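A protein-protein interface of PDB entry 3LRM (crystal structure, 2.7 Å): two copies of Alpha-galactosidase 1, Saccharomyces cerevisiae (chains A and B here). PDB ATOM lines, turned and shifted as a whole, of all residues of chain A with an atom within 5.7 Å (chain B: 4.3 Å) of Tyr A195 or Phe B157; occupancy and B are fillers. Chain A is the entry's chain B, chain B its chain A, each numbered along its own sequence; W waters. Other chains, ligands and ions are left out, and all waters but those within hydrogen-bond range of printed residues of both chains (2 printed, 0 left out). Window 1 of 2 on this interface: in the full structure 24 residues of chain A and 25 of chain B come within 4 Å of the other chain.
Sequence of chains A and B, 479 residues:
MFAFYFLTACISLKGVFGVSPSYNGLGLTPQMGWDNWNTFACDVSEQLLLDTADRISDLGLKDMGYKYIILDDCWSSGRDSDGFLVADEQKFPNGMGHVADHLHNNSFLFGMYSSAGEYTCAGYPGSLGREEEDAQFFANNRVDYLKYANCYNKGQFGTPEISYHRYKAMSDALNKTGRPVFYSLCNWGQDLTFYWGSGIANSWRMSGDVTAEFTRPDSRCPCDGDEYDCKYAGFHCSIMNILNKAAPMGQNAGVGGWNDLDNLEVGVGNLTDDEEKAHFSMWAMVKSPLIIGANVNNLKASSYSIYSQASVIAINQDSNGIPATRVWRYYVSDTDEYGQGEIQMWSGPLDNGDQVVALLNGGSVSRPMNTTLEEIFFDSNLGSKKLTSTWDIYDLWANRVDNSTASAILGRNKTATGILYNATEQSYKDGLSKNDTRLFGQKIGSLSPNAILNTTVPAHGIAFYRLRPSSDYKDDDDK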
ATOM      1  N   THR A 159       2.106 -19.969  24.928  1.00  0.00           N
ATOM      2  CA  THR A 159       2.512 -21.215  24.289  1.00  0.00           C
ATOM      3  C   THR A 159       2.560 -20.978  22.778  1.00  0.00           C
ATOM      4  O   THR A 159       1.918 -20.049  22.285  1.00  0.00           O
ATOM      5  CB  THR A 159       1.561 -22.389  24.616  1.00  0.00           C
ATOM      6  OG1 THR A 159       0.287 -22.158  24.009  1.00  0.00           O
ATOM      7  CG2 THR A 159       1.395 -22.575  26.121  1.00  0.00           C
ATOM      8  N   PRO A 160       3.337 -21.794  22.041  1.00  0.00           N
ATOM      9  CA  PRO A 160       3.360 -21.682  20.585  1.00  0.00           C
ATOM     10  C   PRO A 160       1.968 -21.787  19.950  1.00  0.00           C
ATOM     11  O   PRO A 160       1.609 -20.970  19.105  1.00  0.00           O
ATOM     12  CB  PRO A 160       4.229 -22.869  20.164  1.00  0.00           C
ATOM     13  CG  PRO A 160       5.160 -23.039  21.288  1.00  0.00           C
ATOM     14  CD  PRO A 160       4.366 -22.729  22.524  1.00  0.00           C
ATOM     15  N   GLU A 161       1.188 -22.772  20.380  1.00  0.00           N
ATOM     16  CA  GLU A 161      -0.115 -23.038  19.784  1.00  0.00           C
ATOM     17  C   GLU A 161      -1.055 -21.831  19.794  1.00  0.00           C
ATOM     18  O   GLU A 161      -1.603 -21.460  18.756  1.00  0.00           O
ATOM     19  CB  GLU A 161      -0.777 -24.221  20.478  1.00  0.00           C
ATOM     20  CG  GLU A 161      -2.090 -24.633  19.849  1.00  0.00           C
ATOM     21  CD  GLU A 161      -2.886 -25.578  20.727  1.00  0.00           C
ATOM     22  OE1 GLU A 161      -3.486 -26.528  20.172  1.00  0.00           O
ATOM     23  OE2 GLU A 161      -2.907 -25.372  21.966  1.00  0.00           O
ATOM     24  N   ASP A 191       6.946 -16.931  21.881  1.00  0.00           N
ATOM     25  CA  ASP A 191       6.484 -18.313  21.759  1.00  0.00           C
ATOM     26  C   ASP A 191       7.110 -19.024  20.571  1.00  0.00           C
ATOM     27  O   ASP A 191       6.452 -19.815  19.884  1.00  0.00           O
ATOM     28  CB  ASP A 191       4.951 -18.386  21.729  1.00  0.00           C
ATOM     29  CG  ASP A 191       4.322 -17.882  23.012  1.00  0.00           C
ATOM     30  OD1 ASP A 191       4.821 -18.247  24.094  1.00  0.00           O
ATOM     31  OD2 ASP A 191       3.328 -17.130  22.939  1.00  0.00           O
ATOM     32  N   LEU A 192       8.390 -18.729  20.350  1.00  0.00           N
ATOM     33  CA  LEU A 192       9.229 -19.407  19.354  1.00  0.00           C
ATOM     34  C   LEU A 192       8.679 -19.315  17.924  1.00  0.00           C
ATOM     35  O   LEU A 192       8.424 -20.333  17.274  1.00  0.00           O
ATOM     36  CB  LEU A 192       9.497 -20.868  19.767  1.00  0.00           C
ATOM     37  CG  LEU A 192      10.055 -21.100  21.178  1.00  0.00           C
ATOM     38  CD1 LEU A 192       9.856 -22.531  21.624  1.00  0.00           C
ATOM     39  CD2 LEU A 192      11.513 -20.708  21.280  1.00  0.00           C
ATOM     40  N   THR A 193       8.524 -18.083  17.441  1.00  0.00           N
ATOM     41  CA  THR A 193       7.907 -17.814  16.140  1.00  0.00           C
ATOM     42  C   THR A 193       8.628 -18.490  14.971  1.00  0.00           C
ATOM     43  O   THR A 193       7.988 -18.963  14.037  1.00  0.00           O
ATOM     44  CB  THR A 193       7.790 -16.299  15.871  1.00  0.00           C
ATOM     45  OG1 THR A 193       7.447 -15.620  17.081  1.00  0.00           O
ATOM     46  CG2 THR A 193       6.718 -16.023  14.832  1.00  0.00           C
ATOM     47  N   PHE A 194       9.951 -18.541  15.034  1.00  0.00           N
ATOM     48  CA  PHE A 194      10.759 -19.120  13.962  1.00  0.00           C
ATOM     49  C   PHE A 194      10.312 -20.537  13.580  1.00  0.00           C
ATOM     50  O   PHE A 194      10.548 -20.984  12.463  1.00  0.00           O
ATOM     51  CB  PHE A 194      12.245 -19.100  14.341  1.00  0.00           C
ATOM     52  CG  PHE A 194      12.562 -19.867  15.593  1.00  0.00           C
ATOM     53  CD1 PHE A 194      12.777 -21.240  15.552  1.00  0.00           C
ATOM     54  CD2 PHE A 194      12.649 -19.214  16.818  1.00  0.00           C
ATOM     55  CE1 PHE A 194      13.058 -21.952  16.714  1.00  0.00           C
ATOM     56  CE2 PHE A 194      12.936 -19.920  17.986  1.00  0.00           C
ATOM     57  CZ  PHE A 194      13.138 -21.290  17.936  1.00  0.00           C
ATOM     58  N   TYR A 195       9.661 -21.227  14.511  1.00  0.00           N
ATOM     59  CA  TYR A 195       9.156 -22.578  14.274  1.00  0.00           C
ATOM     60  C   TYR A 195       7.864 -22.614  13.456  1.00  0.00           C
ATOM     61  O   TYR A 195       7.697 -23.473  12.600  1.00  0.00           O
ATOM     62  CB  TYR A 195       8.923 -23.311  15.600  1.00  0.00           C
ATOM     63  CG  TYR A 195      10.107 -24.084  16.159  1.00  0.00           C
ATOM     64  CD1 TYR A 195      10.400 -24.045  17.520  1.00  0.00           C
ATOM     65  CD2 TYR A 195      10.921 -24.858  15.336  1.00  0.00           C
ATOM     66  CE1 TYR A 195      11.472 -24.756  18.050  1.00  0.00           C
ATOM     67  CE2 TYR A 195      12.002 -25.569  15.856  1.00  0.00           C
ATOM     68  CZ  TYR A 195      12.271 -25.512  17.214  1.00  0.00           C
ATOM     69  OH  TYR A 195      13.335 -26.212  17.736  1.00  0.00           O
ATOM     70  N   TRP A 196       6.951 -21.689  13.719  1.00  0.00           N
ATOM     71  CA  TRP A 196       5.601 -21.775  13.162  1.00  0.00           C
ATOM     72  C   TRP A 196       5.211 -20.659  12.182  1.00  0.00           C
ATOM     73  O   TRP A 196       4.105 -20.673  11.627  1.00  0.00           O
ATOM     74  CB  TRP A 196       4.562 -21.883  14.289  1.00  0.00           C
ATOM     75  CG  TRP A 196       4.706 -20.862  15.383  1.00  0.00           C
ATOM     76  CD1 TRP A 196       5.378 -21.018  16.554  1.00  0.00           C
ATOM     77  CD2 TRP A 196       4.158 -19.537  15.409  1.00  0.00           C
ATOM     78  NE1 TRP A 196       5.290 -19.874  17.311  1.00  0.00           N
ATOM     79  CE2 TRP A 196       4.541 -18.951  16.633  1.00  0.00           C
ATOM     80  CE3 TRP A 196       3.382 -18.788  14.519  1.00  0.00           C
ATOM     81  CZ2 TRP A 196       4.174 -17.650  16.991  1.00  0.00           C
ATOM     82  CZ3 TRP A 196       3.019 -17.489  14.877  1.00  0.00           C
ATOM     83  CH2 TRP A 196       3.415 -16.938  16.101  1.00  0.00           C
ATOM     84  N   GLY A 197       6.119 -19.710  11.966  1.00  0.00           N
ATOM     85  CA  GLY A 197       5.862 -18.570  11.081  1.00  0.00           C
ATOM     86  C   GLY A 197       5.661 -18.902   9.609  1.00  0.00           C
ATOM     87  O   GLY A 197       4.722 -18.402   8.982  1.00  0.00           O
ATOM     88  N   SER A 198       6.535 -19.753   9.067  1.00  0.00           N
ATOM     89  CA  SER A 198       6.599 -20.025   7.626  1.00  0.00           C
ATOM     90  C   SER A 198       5.270 -20.417   6.988  1.00  0.00           C
ATOM     91  O   SER A 198       4.958 -19.955   5.895  1.00  0.00           O
ATOM     92  CB  SER A 198       7.653 -21.094   7.312  1.00  0.00           C
ATOM     93  OG  SER A 198       7.166 -22.396   7.578  1.00  0.00           O
ATOM     94  N   ASN A 252      15.766 -21.841  10.380  1.00  0.00           N
ATOM     95  CA  ASN A 252      14.312 -21.853  10.231  1.00  0.00           C
ATOM     96  C   ASN A 252      13.768 -20.763   9.299  1.00  0.00           C
ATOM     97  O   ASN A 252      12.562 -20.505   9.262  1.00  0.00           O
ATOM     98  CB  ASN A 252      13.627 -21.806  11.595  1.00  0.00           C
ATOM     99  CG  ASN A 252      13.614 -23.149  12.279  1.00  0.00           C
ATOM    100  OD1 ASN A 252      14.615 -23.586  12.845  1.00  0.00           O
ATOM    101  ND2 ASN A 252      12.470 -23.811  12.238  1.00  0.00           N
ATOM    102  N   ASN B 153       5.357 -28.159  11.774  1.00  0.00           N
ATOM    103  CA  ASN B 153       4.308 -28.794  12.570  1.00  0.00           C
ATOM    104  C   ASN B 153       3.120 -27.895  12.913  1.00  0.00           C
ATOM    105  O   ASN B 153       2.300 -28.246  13.760  1.00  0.00           O
ATOM    106  CB  ASN B 153       4.914 -29.404  13.838  1.00  0.00           C
ATOM    107  CG  ASN B 153       5.635 -28.380  14.699  1.00  0.00           C
ATOM    108  OD1 ASN B 153       5.204 -27.238  14.802  1.00  0.00           O
ATOM    109  ND2 ASN B 153       6.733 -28.791  15.327  1.00  0.00           N
ATOM    110  N   GLY B 155       2.613 -25.149  14.596  1.00  0.00           N
ATOM    111  CA  GLY B 155       2.496 -24.719  15.985  1.00  0.00           C
ATOM    112  C   GLY B 155       1.997 -25.774  16.956  1.00  0.00           C
ATOM    113  O   GLY B 155       1.610 -25.445  18.076  1.00  0.00           O
ATOM    114  N   GLN B 156       2.008 -27.040  16.543  1.00  0.00           N
ATOM    115  CA  GLN B 156       1.499 -28.130  17.384  1.00  0.00           C
ATOM    116  C   GLN B 156       2.575 -28.736  18.297  1.00  0.00           C
ATOM    117  O   GLN B 156       2.841 -29.938  18.275  1.00  0.00           O
ATOM    118  CB  GLN B 156       0.809 -29.198  16.534  1.00  0.00           C
ATOM    119  CG  GLN B 156      -0.512 -28.744  15.943  1.00  0.00           C
ATOM    120  CD  GLN B 156      -1.255 -29.856  15.231  1.00  0.00           C
ATOM    121  OE1 GLN B 156      -1.376 -30.974  15.738  1.00  0.00           O
ATOM    122  NE2 GLN B 156      -1.773 -29.548  14.049  1.00  0.00           N
ATOM    123  N   PHE B 157       3.180 -27.869  19.099  1.00  0.00           N
ATOM    124  CA  PHE B 157       4.233 -28.222  20.043  1.00  0.00           C
ATOM    125  C   PHE B 157       4.225 -27.156  21.134  1.00  0.00           C
ATOM    126  O   PHE B 157       3.475 -26.182  21.040  1.00  0.00           O
ATOM    127  CB  PHE B 157       5.599 -28.247  19.342  1.00  0.00           C
ATOM    128  CG  PHE B 157       6.133 -26.879  19.008  1.00  0.00           C
ATOM    129  CD1 PHE B 157       7.097 -26.278  19.816  1.00  0.00           C
ATOM    130  CD2 PHE B 157       5.659 -26.183  17.892  1.00  0.00           C
ATOM    131  CE1 PHE B 157       7.586 -25.011  19.519  1.00  0.00           C
ATOM    132  CE2 PHE B 157       6.139 -24.912  17.583  1.00  0.00           C
ATOM    133  CZ  PHE B 157       7.102 -24.323  18.401  1.00  0.00           C
ATOM    134  N   GLY B 158       5.063 -27.332  22.152  1.00  0.00           N
ATOM    135  CA  GLY B 158       5.219 -26.331  23.205  1.00  0.00           C
ATOM    136  C   GLY B 158       4.852 -26.843  24.578  1.00  0.00           C
ATOM    137  O   GLY B 158       5.256 -26.276  25.584  1.00  0.00           O
ATOM    138  N   THR B 159       4.053 -27.899  24.607  1.00  0.00           N
ATOM    139  CA  THR B 159       3.752 -28.642  25.817  1.00  0.00           C
ATOM    140  C   THR B 159       3.875 -30.134  25.482  1.00  0.00           C
ATOM    141  O   THR B 159       3.759 -30.513  24.314  1.00  0.00           O
ATOM    142  CB  THR B 159       2.332 -28.326  26.379  1.00  0.00           C
ATOM    143  OG1 THR B 159       1.325 -28.792  25.476  1.00  0.00           O
ATOM    144  CG2 THR B 159       2.140 -26.841  26.619  1.00  0.00           C
ATOM    145  N   ILE B 162       0.393 -31.712  23.684  1.00  0.00           N
ATOM    146  CA  ILE B 162       0.159 -31.404  22.272  1.00  0.00           C
ATOM    147  C   ILE B 162       1.098 -32.146  21.318  1.00  0.00           C
ATOM    148  O   ILE B 162       0.671 -32.597  20.251  1.00  0.00           O
ATOM    149  CB  ILE B 162       0.162 -29.869  22.008  1.00  0.00           C
ATOM    150  CG1 ILE B 162      -0.255 -29.560  20.566  1.00  0.00           C
ATOM    151  CG2 ILE B 162       1.505 -29.244  22.351  1.00  0.00           C
ATOM    152  CD1 ILE B 162      -0.674 -28.123  20.336  1.00  0.00           C
ATOM    153  N   SER B 163       2.366 -32.279  21.708  1.00  0.00           N
ATOM    154  CA  SER B 163       3.336 -33.062  20.941  1.00  0.00           C
ATOM    155  C   SER B 163       3.007 -34.552  20.989  1.00  0.00           C
ATOM    156  O   SER B 163       3.146 -35.254  19.988  1.00  0.00           O
ATOM    157  CB  SER B 163       4.760 -32.822  21.447  1.00  0.00           C
ATOM    158  OG  SER B 163       5.277 -31.593  20.970  1.00  0.00           O
ATOM    159  N   ARG B 166       0.027 -35.314  18.574  1.00  0.00           N
ATOM    160  CA  ARG B 166       0.493 -35.231  17.194  1.00  0.00           C
ATOM    161  C   ARG B 166       1.217 -36.513  16.770  1.00  0.00           C
ATOM    162  O   ARG B 166       0.999 -37.018  15.672  1.00  0.00           O
ATOM    163  CB  ARG B 166       1.373 -33.995  16.985  1.00  0.00           C
ATOM    164  CG  ARG B 166       1.869 -33.804  15.550  1.00  0.00           C
ATOM    165  CD  ARG B 166       2.292 -32.365  15.257  1.00  0.00           C
ATOM    166  NE  ARG B 166       3.160 -31.806  16.291  1.00  0.00           N
ATOM    167  CZ  ARG B 166       4.484 -31.905  16.309  1.00  0.00           C
ATOM    168  NH1 ARG B 166       5.123 -32.539  15.337  1.00  0.00           N
ATOM    169  NH2 ARG B 166       5.172 -31.360  17.302  1.00  0.00           N
ATOM    170  N   GLN B 190      11.917 -32.621  21.810  1.00  0.00           N
ATOM    171  CA  GLN B 190      11.022 -31.498  22.086  1.00  0.00           C
ATOM    172  C   GLN B 190       9.854 -31.884  22.990  1.00  0.00           C
ATOM    173  O   GLN B 190       9.181 -32.894  22.759  1.00  0.00           O
ATOM    174  CB  GLN B 190      10.491 -30.906  20.782  1.00  0.00           C
ATOM    175  CG  GLN B 190       9.819 -29.553  20.925  1.00  0.00           C
ATOM    176  CD  GLN B 190       9.336 -29.013  19.597  1.00  0.00           C
ATOM    177  OE1 GLN B 190       8.497 -29.623  18.938  1.00  0.00           O
ATOM    178  NE2 GLN B 190       9.864 -27.864  19.194  1.00  0.00           N
ATOM    179  N   ASP B 191       9.636 -31.059  24.014  1.00  0.00           N
ATOM    180  CA  ASP B 191       8.560 -31.239  24.982  1.00  0.00           C
ATOM    181  C   ASP B 191       8.714 -32.523  25.797  1.00  0.00           C
ATOM    182  O   ASP B 191       7.732 -33.222  26.080  1.00  0.00           O
ATOM    183  CB  ASP B 191       7.193 -31.160  24.296  1.00  0.00           C
ATOM    184  CG  ASP B 191       6.942 -29.814  23.652  1.00  0.00           C
ATOM    185  OD1 ASP B 191       7.235 -28.781  24.293  1.00  0.00           O
ATOM    186  OD2 ASP B 191       6.448 -29.787  22.506  1.00  0.00           O
ATOM    187  N   LYS B 231      14.694 -25.781  24.099  1.00  0.00           N
ATOM    188  CA  LYS B 231      13.583 -25.137  23.399  1.00  0.00           C
ATOM    189  C   LYS B 231      13.887 -24.888  21.914  1.00  0.00           C
ATOM    190  O   LYS B 231      12.972 -24.659  21.115  1.00  0.00           O
ATOM    191  CB  LYS B 231      13.182 -23.835  24.100  1.00  0.00           C
ATOM    192  CG  LYS B 231      12.859 -23.985  25.572  1.00  0.00           C
ATOM    193  CD  LYS B 231      11.535 -24.681  25.785  1.00  0.00           C
ATOM    194  CE  LYS B 231      11.294 -24.942  27.253  1.00  0.00           C
ATOM    195  NZ  LYS B 231       9.926 -25.480  27.475  1.00  0.00           N
ATOM    196  N   TYR B 232      15.172 -24.933  21.560  1.00  0.00           N
ATOM    197  CA  TYR B 232      15.616 -24.846  20.172  1.00  0.00           C
ATOM    198  C   TYR B 232      16.650 -25.939  19.922  1.00  0.00           C
ATOM    199  O   TYR B 232      17.855 -25.687  19.975  1.00  0.00           O
ATOM    200  CB  TYR B 232      16.231 -23.472  19.884  1.00  0.00           C
ATOM    201  CG  TYR B 232      16.229 -23.044  18.433  1.00  0.00           C
ATOM    202  CD1 TYR B 232      16.531 -21.733  18.082  1.00  0.00           C
ATOM    203  CD2 TYR B 232      15.908 -23.938  17.412  1.00  0.00           C
ATOM    204  CE1 TYR B 232      16.527 -21.320  16.744  1.00  0.00           C
ATOM    205  CE2 TYR B 232      15.903 -23.544  16.075  1.00  0.00           C
ATOM    206  CZ  TYR B 232      16.210 -22.236  15.747  1.00  0.00           C
ATOM    207  OH  TYR B 232      16.192 -21.851  14.422  1.00  0.00           O
ATOM    208  N   ALA B 233      16.165 -27.150  19.656  1.00  0.00           N
ATOM    209  CA  ALA B 233      17.008 -28.331  19.459  1.00  0.00           C
ATOM    210  C   ALA B 233      18.124 -28.109  18.445  1.00  0.00           C
ATOM    211  O   ALA B 233      19.264 -28.531  18.670  1.00  0.00           O
ATOM    212  CB  ALA B 233      16.162 -29.512  19.056  1.00  0.00           C
HETATM  213  O   HOH W   1       2.050 -24.721  22.463  1.00  0.00           O
HETATM  214  O   HOH W   2       5.508 -24.987  13.898  1.00  0.00           O
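Hydrophobic or aromatic side chains of chain A within 4 Å of the printed part of chain B: Pro A160, Leu A192, Phe A194, Tyr A195 and Trp A196. Of the 14 printed residues of chain B, 8 touch a printed residue of chain A. Hydrophobic or aromatic side chains of chain B that line the printed part of chain A: Phe B157, Ile B162 and Tyr B232. Among the printed residues, no Asp or Glu carboxylate lies within 4 Å of a Lys or Arg side-chain nitrogen of the other chain.
The backbone NH (N) of Gly B155 sits close to the side-chain amide oxygen (OD1) of Asn B153. The side-chain carboxylate (OD2) of Asp B191 sits at hydrogen-bond distance from the backbone NH (N) of Gly B158 (2.8 Å). The backbone carbonyl oxygen (O) of Asp A191 sits at hydrogen-bond distance from the indole nitrogen (NE1) of Trp A196, at 2.8 Å. NE1 of Trp A196 lies within hydrogen-bond range of O of Leu A192, 3.2 Å away. The side-chain amide nitrogen (ND2) of Asn A252 sits close to the backbone carbonyl oxygen (O) of Phe A194 (3.4 Å).
Of the printed residues of chain B, Glu A161 touches Gly B155 and Ile B162. Of the printed residues of chain B, Pro A160 touches Phe B157 and Gly B158. Of the printed residues of chain B, Trp A196 touches Gly B155. Ser A198 touches none of the printed residues of chain B. Asp B191 touches none of the printed residues of chain A. The nearest residue of chain A that does not touch Phe B157 is Trp A196 (4.1 Å).
Pro A160 touches Phe B157 (CB to O, 3.5 Å). Gly B158 touches Pro A160. Lys B231 touches Leu A192. Phe A194 touches Tyr B232 (CE1 to CZ, 3.3 Å). Phe B157 touches Tyr A195 (CZ to CD1, 3.4 Å). Gln B190 touches Tyr A195 (NE2 to CE1, 3.7 Å). CE1 of Tyr A195 touches O of Lys B231 (3.4 Å). Tyr A195 touches Tyr B232. Ala B233 touches Tyr A195. Trp A196 touches Gly B155.
The side-chain hydroxyl of Tyr B232 lies within hydrogen-bond range of the side-chain amide oxygen of Asn A252 (2.8 Å).
Positions printed for both chains: 159 and 191. Of the 14 pairs that touch across the chains among the printed residues, none has its exchanged pair printed and touching as well.
Water W2 lies within hydrogen-bond range of the side-chain amide oxygen of Asn B153 (2.4 Å), the backbone carbonyl oxygen of Tyr A195 (3.0 Å) and the backbone NH of Gly B155 (3.0 Å). Water W1 lies within hydrogen-bond range of the backbone carbonyl oxygen (O) of Phe B157 (2.5 Å), the backbone NH (N) of Glu A161 (3.0 Å) and the side-chain hydroxyl (OG1) of Thr A159 (3.5 Å).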
